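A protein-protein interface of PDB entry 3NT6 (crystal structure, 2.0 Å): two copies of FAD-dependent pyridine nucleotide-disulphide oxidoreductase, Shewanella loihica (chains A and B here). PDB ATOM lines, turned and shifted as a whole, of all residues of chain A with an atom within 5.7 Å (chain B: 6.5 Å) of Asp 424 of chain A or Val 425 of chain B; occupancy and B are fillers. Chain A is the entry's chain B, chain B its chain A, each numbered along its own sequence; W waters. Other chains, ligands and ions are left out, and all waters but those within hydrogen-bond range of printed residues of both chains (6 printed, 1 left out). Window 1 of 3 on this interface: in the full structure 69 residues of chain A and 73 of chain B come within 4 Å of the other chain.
Val 425 of chain B touches two residues of chain A. Of the printed residues of chain A, Tyr 450 of chain B touches Asp 420. Of the printed residues of chain A, Asp 424 of chain B touches Lys 421 and Val 425. Of the printed residues of chain A, Leu 444 of chain B touches Thr 348 (3.6 Å), Asp 424 (3.5 Å) and Val 428 (3.7 Å). Ile 457 of chain B touches none of the printed residues of chain A. Arg 422 of chain A touches none of the printed residues of chain B.
The backbone carbonyl oxygen (O) of Glu 443 of chain B lies within hydrogen-bond range of the side-chain hydroxyl (OG1) of Thr 348 of chain A, at 2.8 Å. The side-chain amino group (NZ) of Lys 421 of chain A lies within salt-bridge range of the side-chain carboxylate (OD2) of Asp 420 of chain B. NZ of Lys 421 of chain B is in salt-bridge range of OD2 of Asp 424 of chain A, at 3.98 Å. OD1 of Asp 424 of chain A lies within hydrogen-bond range of N of Ser 445 of chain B. OD2 of Asp 420 of chain A is in salt-bridge range of NZ of Lys 421 of chain B (2.9 Å).
Asp 420 of chain A touches Lys 421 of chain B, and with the chains exchanged Lys 421 of chain A touches Asp 420 of chain B. Lys 421 of chain B touches its own counterpart, Lys 421 of chain A. Lys 421 of chain A touches Asp 424 of chain B, and with the chains exchanged Asp 424 of chain A touches Lys 421 of chain B. Ala 429 of chain A touches Val 428 of chain B, but with the chains exchanged Val 428 of chain A does not touch Ala 429 of chain B (4.04 Å). Of the 20 pairs that touch across the chains among the printed residues, 9 have their exchanged pair printed and touching as well.
Water W1 bridges OD2 of Asp 424 of chain A (2.6 Å) and OD2 of Asp 455 of chain B (3.4 Å). Water W5 bridges O of Thr 348 of chain A (2.6 Å) and N of Tyr 446 of chain B (3.1 Å). Water W2 lies within hydrogen-bond range of NZ of Lys 421 of chain B (2.7 Å), O of Ser 445 of chain B (2.7 Å) and OD2 of Asp 424 of chain A (2.7 Å). Water W4 bridges NZ of Lys 421 of chain A and OD2 of Asp 424 of chain B. Water W3 bridges the backbone NH (N) of Glu 443 of chain B and the backbone carbonyl oxygen (O) of Ala 427 of chain A. Water W6 bridges the side-chain carboxylate (OD2) of Asp 424 of chain B (3.0 Å) and the guanidinium group (NE) of Arg 422 of chain A (3.2 Å).
Hydrophobic or aromatic side chains of chain B that line the printed part of chain A: Val 425, Val 428, Leu 442 and Leu 444. Along chain B the printed residues that touch a printed residue of chain A span positions 420 to 450. Of the 12 printed residues of chain A, 9 touch a printed residue of chain B. Printed residues of chain A that touch a printed residue of chain B: Thr 348, Asp 420, Lys 421, Ile 423, Asp 424, Val 425, Ala 427, Val 428 and Ala 429. Hydrophobic or aromatic side chains of chain A within 4 Å of the printed part of chain B: Ile 423, Val 425, Ala 427 and Val 428. Among the printed residues, 20 pairs touch across the chains. Among the printed residues, Asp or Glu carboxylates within 4 Å of a Lys or Arg side-chain nitrogen of the other chain: Asp 420 of chain A with Lys 421 of chain B (2.9 Å), Lys 421 of chain A with Asp 420 of chain B (2.5 Å) and Asp 424 of chain A with Lys 421 of chain B (3.98 Å).
NZ of Lys 421 of chain B sits at hydrogen-bond distance from O of Tyr 450 of chain B, at 2.7 Å.
N of Ser 445 of chain B touches CG2 of Thr 348 of chain A, 3.4 Å away. N of Lys 421 of chain A touches CD of Lys 421 of chain B, at 3.9 Å. Lys 421 of chain A touches Asp 424 of chain B. Asp 424 of chain A touches Val 425 of chain B (CB to CG2, 3.7 Å). OD2 of Asp 424 of chain A touches CB of Leu 444 of chain B, at 3.5 Å. Val 425 of chain A touches Asp 424 of chain B. CG2 of Val 428 of chain B touches CG1 of Val 425 of chain A, 3.5 Å away. Glu 443 of chain B touches Ala 427 of chain A (O to CB, 3.5 Å). Val 425 of chain B touches Val 428 of chain A. Leu 442 of chain B touches Val 428 of chain A.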
ATOM      1  N   THR A 348       5.567  19.338 -13.312  1.00  0.00           N
ATOM      2  CA  THR A 348       5.337  19.963 -12.012  1.00  0.00           C
ATOM      3  C   THR A 348       3.833  20.079 -11.639  1.00  0.00           C
ATOM      4  O   THR A 348       3.061  20.676 -12.397  1.00  0.00           O
ATOM      5  CB  THR A 348       5.910  21.361 -12.076  1.00  0.00           C
ATOM      6  OG1 THR A 348       7.267  21.265 -12.588  1.00  0.00           O
ATOM      7  CG2 THR A 348       5.915  22.026 -10.690  1.00  0.00           C
ATOM      8  N   ILE A 419       4.151  23.931   0.774  1.00  0.00           N
ATOM      9  CA  ILE A 419       4.388  22.882  -0.270  1.00  0.00           C
ATOM     10  C   ILE A 419       4.725  23.438  -1.652  1.00  0.00           C
ATOM     11  O   ILE A 419       5.744  22.994  -2.211  1.00  0.00           O
ATOM     12  CB  ILE A 419       3.211  21.804  -0.363  1.00  0.00           C
ATOM     13  CG1 ILE A 419       2.927  21.226   1.047  1.00  0.00           C
ATOM     14  CG2 ILE A 419       3.448  20.792  -1.493  1.00  0.00           C
ATOM     15  CD1 ILE A 419       4.195  20.796   1.761  1.00  0.00           C
ATOM     16  N   ASP A 420       3.870  24.355  -2.156  1.00  0.00           N
ATOM     17  CA  ASP A 420       4.070  25.127  -3.423  1.00  0.00           C
ATOM     18  C   ASP A 420       5.465  25.741  -3.454  1.00  0.00           C
ATOM     19  O   ASP A 420       6.129  25.551  -4.423  1.00  0.00           O
ATOM     20  CB  ASP A 420       3.046  26.208  -3.730  1.00  0.00           C
ATOM     21  CG  ASP A 420       2.869  27.239  -2.564  1.00  0.00           C
ATOM     22  OD1 ASP A 420       3.178  26.920  -1.397  1.00  0.00           O
ATOM     23  OD2 ASP A 420       2.457  28.379  -2.834  1.00  0.00           O
ATOM     24  N   LYS A 421       5.907  26.444  -2.409  1.00  0.00           N
ATOM     25  CA  LYS A 421       7.306  26.901  -2.353  1.00  0.00           C
ATOM     26  C   LYS A 421       8.433  25.812  -2.535  1.00  0.00           C
ATOM     27  O   LYS A 421       9.342  25.964  -3.380  1.00  0.00           O
ATOM     28  CB  LYS A 421       7.600  27.793  -1.083  1.00  0.00           C
ATOM     29  CG  LYS A 421       9.126  28.062  -0.898  1.00  0.00           C
ATOM     30  CD  LYS A 421       9.320  29.207   0.120  1.00  0.00           C
ATOM     31  CE  LYS A 421       8.937  28.712   1.557  1.00  0.00           C
ATOM     32  NZ  LYS A 421       9.177  29.848   2.506  1.00  0.00           N
ATOM     33  N   ARG A 422       8.413  24.753  -1.779  1.00  0.00           N
ATOM     34  CA  ARG A 422       9.436  23.666  -1.957  1.00  0.00           C
ATOM     35  C   ARG A 422       9.452  22.984  -3.328  1.00  0.00           C
ATOM     36  O   ARG A 422      10.506  22.828  -3.911  1.00  0.00           O
ATOM     37  CB  ARG A 422       9.274  22.532  -0.879  1.00  0.00           C
ATOM     38  CG  ARG A 422       9.828  22.912   0.511  1.00  0.00           C
ATOM     39  CD  ARG A 422       9.750  24.459   0.723  1.00  0.00           C
ATOM     40  NE  ARG A 422      10.254  24.916   2.055  1.00  0.00           N
ATOM     41  CZ  ARG A 422       9.505  25.339   3.070  1.00  0.00           C
ATOM     42  NH1 ARG A 422       8.163  25.335   2.920  1.00  0.00           N
ATOM     43  NH2 ARG A 422      10.077  25.898   4.183  1.00  0.00           N
ATOM     44  N   ILE A 423       8.283  22.797  -3.932  1.00  0.00           N
ATOM     45  CA  ILE A 423       8.210  22.136  -5.296  1.00  0.00           C
ATOM     46  C   ILE A 423       8.684  23.096  -6.366  1.00  0.00           C
ATOM     47  O   ILE A 423       9.362  22.680  -7.320  1.00  0.00           O
ATOM     48  CB  ILE A 423       6.811  21.685  -5.587  1.00  0.00           C
ATOM     49  CG1 ILE A 423       6.476  20.519  -4.596  1.00  0.00           C
ATOM     50  CG2 ILE A 423       6.661  21.221  -7.062  1.00  0.00           C
ATOM     51  CD1 ILE A 423       7.486  19.318  -4.607  1.00  0.00           C
ATOM     52  N   ASP A 424       8.382  24.386  -6.183  1.00  0.00           N
ATOM     53  CA  ASP A 424       8.835  25.431  -7.106  1.00  0.00           C
ATOM     54  C   ASP A 424      10.328  25.534  -7.088  1.00  0.00           C
ATOM     55  O   ASP A 424      10.961  25.605  -8.142  1.00  0.00           O
ATOM     56  CB  ASP A 424       8.135  26.766  -6.812  1.00  0.00           C
ATOM     57  CG  ASP A 424       6.648  26.778  -7.356  1.00  0.00           C
ATOM     58  OD1 ASP A 424       6.103  25.689  -7.706  1.00  0.00           O
ATOM     59  OD2 ASP A 424       6.038  27.882  -7.486  1.00  0.00           O
ATOM     60  N   VAL A 425      10.903  25.530  -5.889  1.00  0.00           N
ATOM     61  CA  VAL A 425      12.352  25.610  -5.805  1.00  0.00           C
ATOM     62  C   VAL A 425      13.016  24.401  -6.465  1.00  0.00           C
ATOM     63  O   VAL A 425      14.012  24.517  -7.239  1.00  0.00           O
ATOM     64  CB  VAL A 425      12.857  25.825  -4.341  1.00  0.00           C
ATOM     65  CG1 VAL A 425      14.364  25.410  -4.231  1.00  0.00           C
ATOM     66  CG2 VAL A 425      12.596  27.326  -3.863  1.00  0.00           C
ATOM     67  N   MET A 426      12.540  23.225  -6.097  1.00  0.00           N
ATOM     68  CA  MET A 426      13.033  22.002  -6.855  1.00  0.00           C
ATOM     69  C   MET A 426      12.885  21.985  -8.421  1.00  0.00           C
ATOM     70  O   MET A 426      13.729  21.444  -9.115  1.00  0.00           O
ATOM     71  CB  MET A 426      12.308  20.742  -6.297  1.00  0.00           C
ATOM     72  CG  MET A 426      12.851  20.387  -4.877  1.00  0.00           C
ATOM     73  SD  MET A 426      14.788  20.429  -4.637  1.00  0.00           S
ATOM     74  CE  MET A 426      15.163  19.128  -6.075  1.00  0.00           C
ATOM     75  N   ALA A 427      11.755  22.479  -8.944  1.00  0.00           N
ATOM     76  CA  ALA A 427      11.499  22.590 -10.378  1.00  0.00           C
ATOM     77  C   ALA A 427      12.503  23.517 -10.941  1.00  0.00           C
ATOM     78  O   ALA A 427      13.077  23.166 -11.948  1.00  0.00           O
ATOM     79  CB  ALA A 427      10.116  23.120 -10.630  1.00  0.00           C
ATOM     80  N   VAL A 428      12.789  24.664 -10.263  1.00  0.00           N
ATOM     81  CA  VAL A 428      13.839  25.527 -10.725  1.00  0.00           C
ATOM     82  C   VAL A 428      15.241  24.831 -10.698  1.00  0.00           C
ATOM     83  O   VAL A 428      15.985  24.847 -11.704  1.00  0.00           O
ATOM     84  CB  VAL A 428      13.904  26.880  -9.977  1.00  0.00           C
ATOM     85  CG1 VAL A 428      14.945  27.770 -10.832  1.00  0.00           C
ATOM     86  CG2 VAL A 428      12.510  27.469 -10.011  1.00  0.00           C
ATOM     87  N   ALA A 429      15.570  24.186  -9.580  1.00  0.00           N
ATOM     88  CA  ALA A 429      16.922  23.579  -9.465  1.00  0.00           C
ATOM     89  C   ALA A 429      17.142  22.546 -10.532  1.00  0.00           C
ATOM     90  O   ALA A 429      18.180  22.545 -11.175  1.00  0.00           O
ATOM     91  CB  ALA A 429      17.150  22.939  -8.021  1.00  0.00           C
ATOM     92  N   ASP B 420       7.783  35.039  -0.010  1.00  0.00           N
ATOM     93  CA  ASP B 420       8.941  34.101   0.288  1.00  0.00           C
ATOM     94  C   ASP B 420       9.186  33.138  -0.891  1.00  0.00           C
ATOM     95  O   ASP B 420      10.362  32.836  -1.268  1.00  0.00           O
ATOM     96  CB  ASP B 420       8.827  33.391   1.673  1.00  0.00           C
ATOM     97  CG  ASP B 420       7.442  32.523   1.850  1.00  0.00           C
ATOM     98  OD1 ASP B 420       6.423  32.820   1.153  1.00  0.00           O
ATOM     99  OD2 ASP B 420       7.398  31.565   2.690  1.00  0.00           O
ATOM    100  N   LYS B 421       8.098  32.723  -1.571  1.00  0.00           N
ATOM    101  CA  LYS B 421       8.208  31.751  -2.695  1.00  0.00           C
ATOM    102  C   LYS B 421       8.846  32.382  -3.955  1.00  0.00           C
ATOM    103  O   LYS B 421       9.524  31.746  -4.656  1.00  0.00           O
ATOM    104  CB  LYS B 421       6.753  31.205  -3.094  1.00  0.00           C
ATOM    105  CG  LYS B 421       6.783  30.399  -4.389  1.00  0.00           C
ATOM    106  CD  LYS B 421       5.506  29.550  -4.778  1.00  0.00           C
ATOM    107  CE  LYS B 421       4.282  30.409  -4.958  1.00  0.00           C
ATOM    108  NZ  LYS B 421       3.079  29.546  -5.406  1.00  0.00           N
ATOM    109  N   ARG B 422       8.471  33.609  -4.295  1.00  0.00           N
ATOM    110  CA  ARG B 422       9.077  34.280  -5.454  1.00  0.00           C
ATOM    111  C   ARG B 422      10.530  34.612  -5.240  1.00  0.00           C
ATOM    112  O   ARG B 422      11.309  34.408  -6.144  1.00  0.00           O
ATOM    113  CB  ARG B 422       8.275  35.626  -5.836  1.00  0.00           C
ATOM    114  CG  ARG B 422       6.968  35.394  -6.760  1.00  0.00           C
ATOM    115  CD  ARG B 422       6.267  34.165  -6.339  1.00  0.00           C
ATOM    116  NE  ARG B 422       5.108  33.651  -7.095  1.00  0.00           N
ATOM    117  CZ  ARG B 422       3.871  33.572  -6.648  1.00  0.00           C
ATOM    118  NH1 ARG B 422       3.610  34.033  -5.481  1.00  0.00           N
ATOM    119  NH2 ARG B 422       2.927  32.937  -7.388  1.00  0.00           N
ATOM    120  N   ILE B 423      10.902  35.081  -4.057  1.00  0.00           N
ATOM    121  CA  ILE B 423      12.321  35.327  -3.718  1.00  0.00           C
ATOM    122  C   ILE B 423      13.207  34.087  -3.703  1.00  0.00           C
ATOM    123  O   ILE B 423      14.382  34.125  -4.240  1.00  0.00           O
ATOM    124  CB  ILE B 423      12.387  36.063  -2.394  1.00  0.00           C
ATOM    125  CG1 ILE B 423      11.705  37.388  -2.659  1.00  0.00           C
ATOM    126  CG2 ILE B 423      13.884  36.406  -1.914  1.00  0.00           C
ATOM    127  CD1 ILE B 423      12.429  38.057  -3.914  1.00  0.00           C
ATOM    128  N   ASP B 424      12.637  32.998  -3.213  1.00  0.00           N
ATOM    129  CA  ASP B 424      13.311  31.718  -3.164  1.00  0.00           C
ATOM    130  C   ASP B 424      13.491  31.157  -4.569  1.00  0.00           C
ATOM    131  O   ASP B 424      14.586  30.612  -4.879  1.00  0.00           O
ATOM    132  CB  ASP B 424      12.594  30.651  -2.310  1.00  0.00           C
ATOM    133  CG  ASP B 424      12.754  30.890  -0.776  1.00  0.00           C
ATOM    134  OD1 ASP B 424      13.134  32.019  -0.308  1.00  0.00           O
ATOM    135  OD2 ASP B 424      12.484  29.891  -0.042  1.00  0.00           O
ATOM    136  N   VAL B 425      12.455  31.296  -5.417  1.00  0.00           N
ATOM    137  CA  VAL B 425      12.686  30.863  -6.834  1.00  0.00           C
ATOM    138  C   VAL B 425      13.831  31.668  -7.556  1.00  0.00           C
ATOM    139  O   VAL B 425      14.739  31.119  -8.121  1.00  0.00           O
ATOM    140  CB  VAL B 425      11.406  30.866  -7.623  1.00  0.00           C
ATOM    141  CG1 VAL B 425      11.684  30.770  -9.072  1.00  0.00           C
ATOM    142  CG2 VAL B 425      10.487  29.631  -7.241  1.00  0.00           C
ATOM    143  N   MET B 426      13.792  33.013  -7.462  1.00  0.00           N
ATOM    144  CA  MET B 426      14.884  33.892  -8.032  1.00  0.00           C
ATOM    145  C   MET B 426      16.208  33.647  -7.406  1.00  0.00           C
ATOM    146  O   MET B 426      17.244  33.665  -8.084  1.00  0.00           O
ATOM    147  CB  MET B 426      14.481  35.355  -7.728  1.00  0.00           C
ATOM    148  CG  MET B 426      13.242  35.808  -8.518  1.00  0.00           C
ATOM    149  SD  MET B 426      13.434  35.295 -10.431  1.00  0.00           S
ATOM    150  CE  MET B 426      15.196  36.166 -10.827  1.00  0.00           C
ATOM    151  N   ALA B 427      16.216  33.325  -6.111  1.00  0.00           N
ATOM    152  CA  ALA B 427      17.506  32.974  -5.459  1.00  0.00           C
ATOM    153  C   ALA B 427      18.100  31.749  -6.074  1.00  0.00           C
ATOM    154  O   ALA B 427      19.354  31.716  -6.379  1.00  0.00           O
ATOM    155  CB  ALA B 427      17.346  32.816  -3.886  1.00  0.00           C
ATOM    156  N   VAL B 428      17.254  30.718  -6.331  1.00  0.00           N
ATOM    157  CA  VAL B 428      17.841  29.507  -6.881  1.00  0.00           C
ATOM    158  C   VAL B 428      18.195  29.794  -8.302  1.00  0.00           C
ATOM    159  O   VAL B 428      19.192  29.306  -8.740  1.00  0.00           O
ATOM    160  CB  VAL B 428      16.861  28.313  -6.874  1.00  0.00           C
ATOM    161  CG1 VAL B 428      17.337  27.038  -7.696  1.00  0.00           C
ATOM    162  CG2 VAL B 428      16.375  28.042  -5.473  1.00  0.00           C
ATOM    163  N   ALA B 429      17.373  30.524  -9.053  1.00  0.00           N
ATOM    164  CA  ALA B 429      17.726  30.687 -10.528  1.00  0.00           C
ATOM    165  C   ALA B 429      18.997  31.453 -10.656  1.00  0.00           C
ATOM    166  O   ALA B 429      19.780  31.150 -11.528  1.00  0.00           O
ATOM    167  CB  ALA B 429      16.620  31.416 -11.322  1.00  0.00           C
ATOM    168  N   GLN B 430      19.166  32.509  -9.852  1.00  0.00           N
ATOM    169  CA  GLN B 430      20.428  33.286  -9.913  1.00  0.00           C
ATOM    170  C   GLN B 430      21.625  32.402  -9.528  1.00  0.00           C
ATOM    171  O   GLN B 430      22.627  32.345 -10.253  1.00  0.00           O
ATOM    172  CB  GLN B 430      20.349  34.524  -9.011  1.00  0.00           C
ATOM    173  CG  GLN B 430      21.758  35.215  -8.907  1.00  0.00           C
ATOM    174  CD  GLN B 430      21.635  36.445  -8.103  1.00  0.00           C
ATOM    175  OE1 GLN B 430      21.310  36.369  -6.923  1.00  0.00           O
ATOM    176  NE2 GLN B 430      21.807  37.621  -8.737  1.00  0.00           N
ATOM    177  N   LEU B 439      14.402  32.015 -17.773  1.00  0.00           N
ATOM    178  CA  LEU B 439      13.346  32.158 -16.794  1.00  0.00           C
ATOM    179  C   LEU B 439      11.961  32.002 -17.388  1.00  0.00           C
ATOM    180  O   LEU B 439      11.062  31.660 -16.698  1.00  0.00           O
ATOM    181  CB  LEU B 439      13.404  33.508 -16.099  1.00  0.00           C
ATOM    182  CG  LEU B 439      14.439  33.846 -15.044  1.00  0.00           C
ATOM    183  CD1 LEU B 439      14.241  35.171 -14.477  1.00  0.00           C
ATOM    184  CD2 LEU B 439      14.440  32.877 -13.979  1.00  0.00           C
ATOM    185  N   LEU B 442      10.456  28.494 -16.989  1.00  0.00           N
ATOM    186  CA  LEU B 442      10.186  27.823 -15.720  1.00  0.00           C
ATOM    187  C   LEU B 442       8.761  27.174 -15.647  1.00  0.00           C
ATOM    188  O   LEU B 442       7.781  27.707 -16.202  1.00  0.00           O
ATOM    189  CB  LEU B 442      10.405  28.759 -14.542  1.00  0.00           C
ATOM    190  CG  LEU B 442      11.849  29.101 -14.239  1.00  0.00           C
ATOM    191  CD1 LEU B 442      12.060  30.156 -13.096  1.00  0.00           C
ATOM    192  CD2 LEU B 442      12.844  27.898 -14.003  1.00  0.00           C
ATOM    193  N   GLU B 443       8.702  25.964 -15.034  1.00  0.00           N
ATOM    194  CA  GLU B 443       7.516  25.196 -14.994  1.00  0.00           C
ATOM    195  C   GLU B 443       7.143  25.049 -13.519  1.00  0.00           C
ATOM    196  O   GLU B 443       7.585  24.084 -12.858  1.00  0.00           O
ATOM    197  CB  GLU B 443       7.780  23.859 -15.610  1.00  0.00           C
ATOM    198  CG  GLU B 443       6.505  23.071 -15.709  1.00  0.00           C
ATOM    199  CD  GLU B 443       6.668  21.728 -16.270  1.00  0.00           C
ATOM    200  OE1 GLU B 443       7.646  21.561 -17.037  1.00  0.00           O
ATOM    201  OE2 GLU B 443       5.781  20.893 -16.008  1.00  0.00           O
ATOM    202  N   LEU B 444       6.389  26.008 -12.984  1.00  0.00           N
ATOM    203  CA  LEU B 444       6.109  26.027 -11.535  1.00  0.00           C
ATOM    204  C   LEU B 444       4.702  25.393 -11.257  1.00  0.00           C
ATOM    205  O   LEU B 444       3.971  25.148 -12.227  1.00  0.00           O
ATOM    206  CB  LEU B 444       6.305  27.412 -10.956  1.00  0.00           C
ATOM    207  CG  LEU B 444       7.677  28.096 -11.303  1.00  0.00           C
ATOM    208  CD1 LEU B 444       7.650  29.380 -10.568  1.00  0.00           C
ATOM    209  CD2 LEU B 444       8.876  27.148 -10.872  1.00  0.00           C
ATOM    210  N   SER B 445       4.433  25.016  -9.985  1.00  0.00           N
ATOM    211  CA  SER B 445       3.175  24.397  -9.549  1.00  0.00           C
ATOM    212  C   SER B 445       2.002  25.317  -9.864  1.00  0.00           C
ATOM    213  O   SER B 445       2.037  26.477  -9.441  1.00  0.00           O
ATOM    214  CB  SER B 445       3.163  24.375  -8.019  1.00  0.00           C
ATOM    215  OG  SER B 445       4.160  23.511  -7.499  1.00  0.00           O
ATOM    216  N   TYR B 446       0.979  24.811 -10.528  1.00  0.00           N
ATOM    217  CA  TYR B 446      -0.285  25.514 -10.681  1.00  0.00           C
ATOM    218  C   TYR B 446      -1.529  24.675 -10.283  1.00  0.00           C
ATOM    219  O   TYR B 446      -1.844  23.655 -10.956  1.00  0.00           O
ATOM    220  CB  TYR B 446      -0.460  25.925 -12.117  1.00  0.00           C
ATOM    221  CG  TYR B 446      -1.812  26.521 -12.268  1.00  0.00           C
ATOM    222  CD1 TYR B 446      -2.655  26.049 -13.235  1.00  0.00           C
ATOM    223  CD2 TYR B 446      -2.277  27.531 -11.367  1.00  0.00           C
ATOM    224  CE1 TYR B 446      -3.961  26.566 -13.360  1.00  0.00           C
ATOM    225  CE2 TYR B 446      -3.586  28.021 -11.475  1.00  0.00           C
ATOM    226  CZ  TYR B 446      -4.398  27.563 -12.498  1.00  0.00           C
ATOM    227  OH  TYR B 446      -5.687  28.074 -12.684  1.00  0.00           O
ATOM    228  N   TYR B 450      -2.882  28.027  -5.088  1.00  0.00           N
ATOM    229  CA  TYR B 450      -1.461  28.136  -4.846  1.00  0.00           C
ATOM    230  C   TYR B 450      -0.709  28.892  -5.895  1.00  0.00           C
ATOM    231  O   TYR B 450       0.378  29.381  -5.608  1.00  0.00           O
ATOM    232  CB  TYR B 450      -0.834  26.728  -4.864  1.00  0.00           C
ATOM    233  CG  TYR B 450      -1.485  25.791  -3.827  1.00  0.00           C
ATOM    234  CD1 TYR B 450      -1.485  26.113  -2.439  1.00  0.00           C
ATOM    235  CD2 TYR B 450      -2.120  24.629  -4.238  1.00  0.00           C
ATOM    236  CE1 TYR B 450      -2.153  25.234  -1.425  1.00  0.00           C
ATOM    237  CE2 TYR B 450      -2.737  23.746  -3.277  1.00  0.00           C
ATOM    238  CZ  TYR B 450      -2.756  24.051  -1.944  1.00  0.00           C
ATOM    239  OH  TYR B 450      -3.369  23.140  -1.138  1.00  0.00           O
ATOM    240  N   ASP B 455       3.179  32.071 -13.897  1.00  0.00           N
ATOM    241  CA  ASP B 455       3.540  32.669 -12.615  1.00  0.00           C
ATOM    242  C   ASP B 455       3.988  34.115 -12.730  1.00  0.00           C
ATOM    243  O   ASP B 455       4.459  34.570 -13.822  1.00  0.00           O
ATOM    244  CB  ASP B 455       4.683  31.879 -11.933  1.00  0.00           C
ATOM    245  CG  ASP B 455       4.857  32.288 -10.417  1.00  0.00           C
ATOM    246  OD1 ASP B 455       3.934  31.959  -9.658  1.00  0.00           O
ATOM    247  OD2 ASP B 455       5.839  32.953 -10.001  1.00  0.00           O
ATOM    248  N   ILE B 457       6.788  35.053 -11.805  1.00  0.00           N
ATOM    249  CA  ILE B 457       8.153  34.952 -12.327  1.00  0.00           C
ATOM    250  C   ILE B 457       8.124  34.740 -13.856  1.00  0.00           C
ATOM    251  O   ILE B 457       8.971  35.315 -14.566  1.00  0.00           O
ATOM    252  CB  ILE B 457       8.875  33.714 -11.660  1.00  0.00           C
ATOM    253  CG1 ILE B 457       9.006  33.810 -10.085  1.00  0.00           C
ATOM    254  CG2 ILE B 457      10.268  33.374 -12.329  1.00  0.00           C
ATOM    255  CD1 ILE B 457       9.358  35.081  -9.634  1.00  0.00           C
HETATM  256  O   HOH W   1       6.448  30.428  -7.736  1.00  0.00           O
HETATM  257  O   HOH W   2       3.301  27.972  -7.546  1.00  0.00           O
HETATM  258  O   HOH W   3      10.898  24.622 -13.686  1.00  0.00           O
HETATM  259  O   HOH W   4      11.900  30.455   2.641  1.00  0.00           O
HETATM  260  O   HOH W   5       0.954  22.261 -12.325  1.00  0.00           O
HETATM  261  O   HOH W   6      12.153  26.936   0.500  1.00  0.00           O
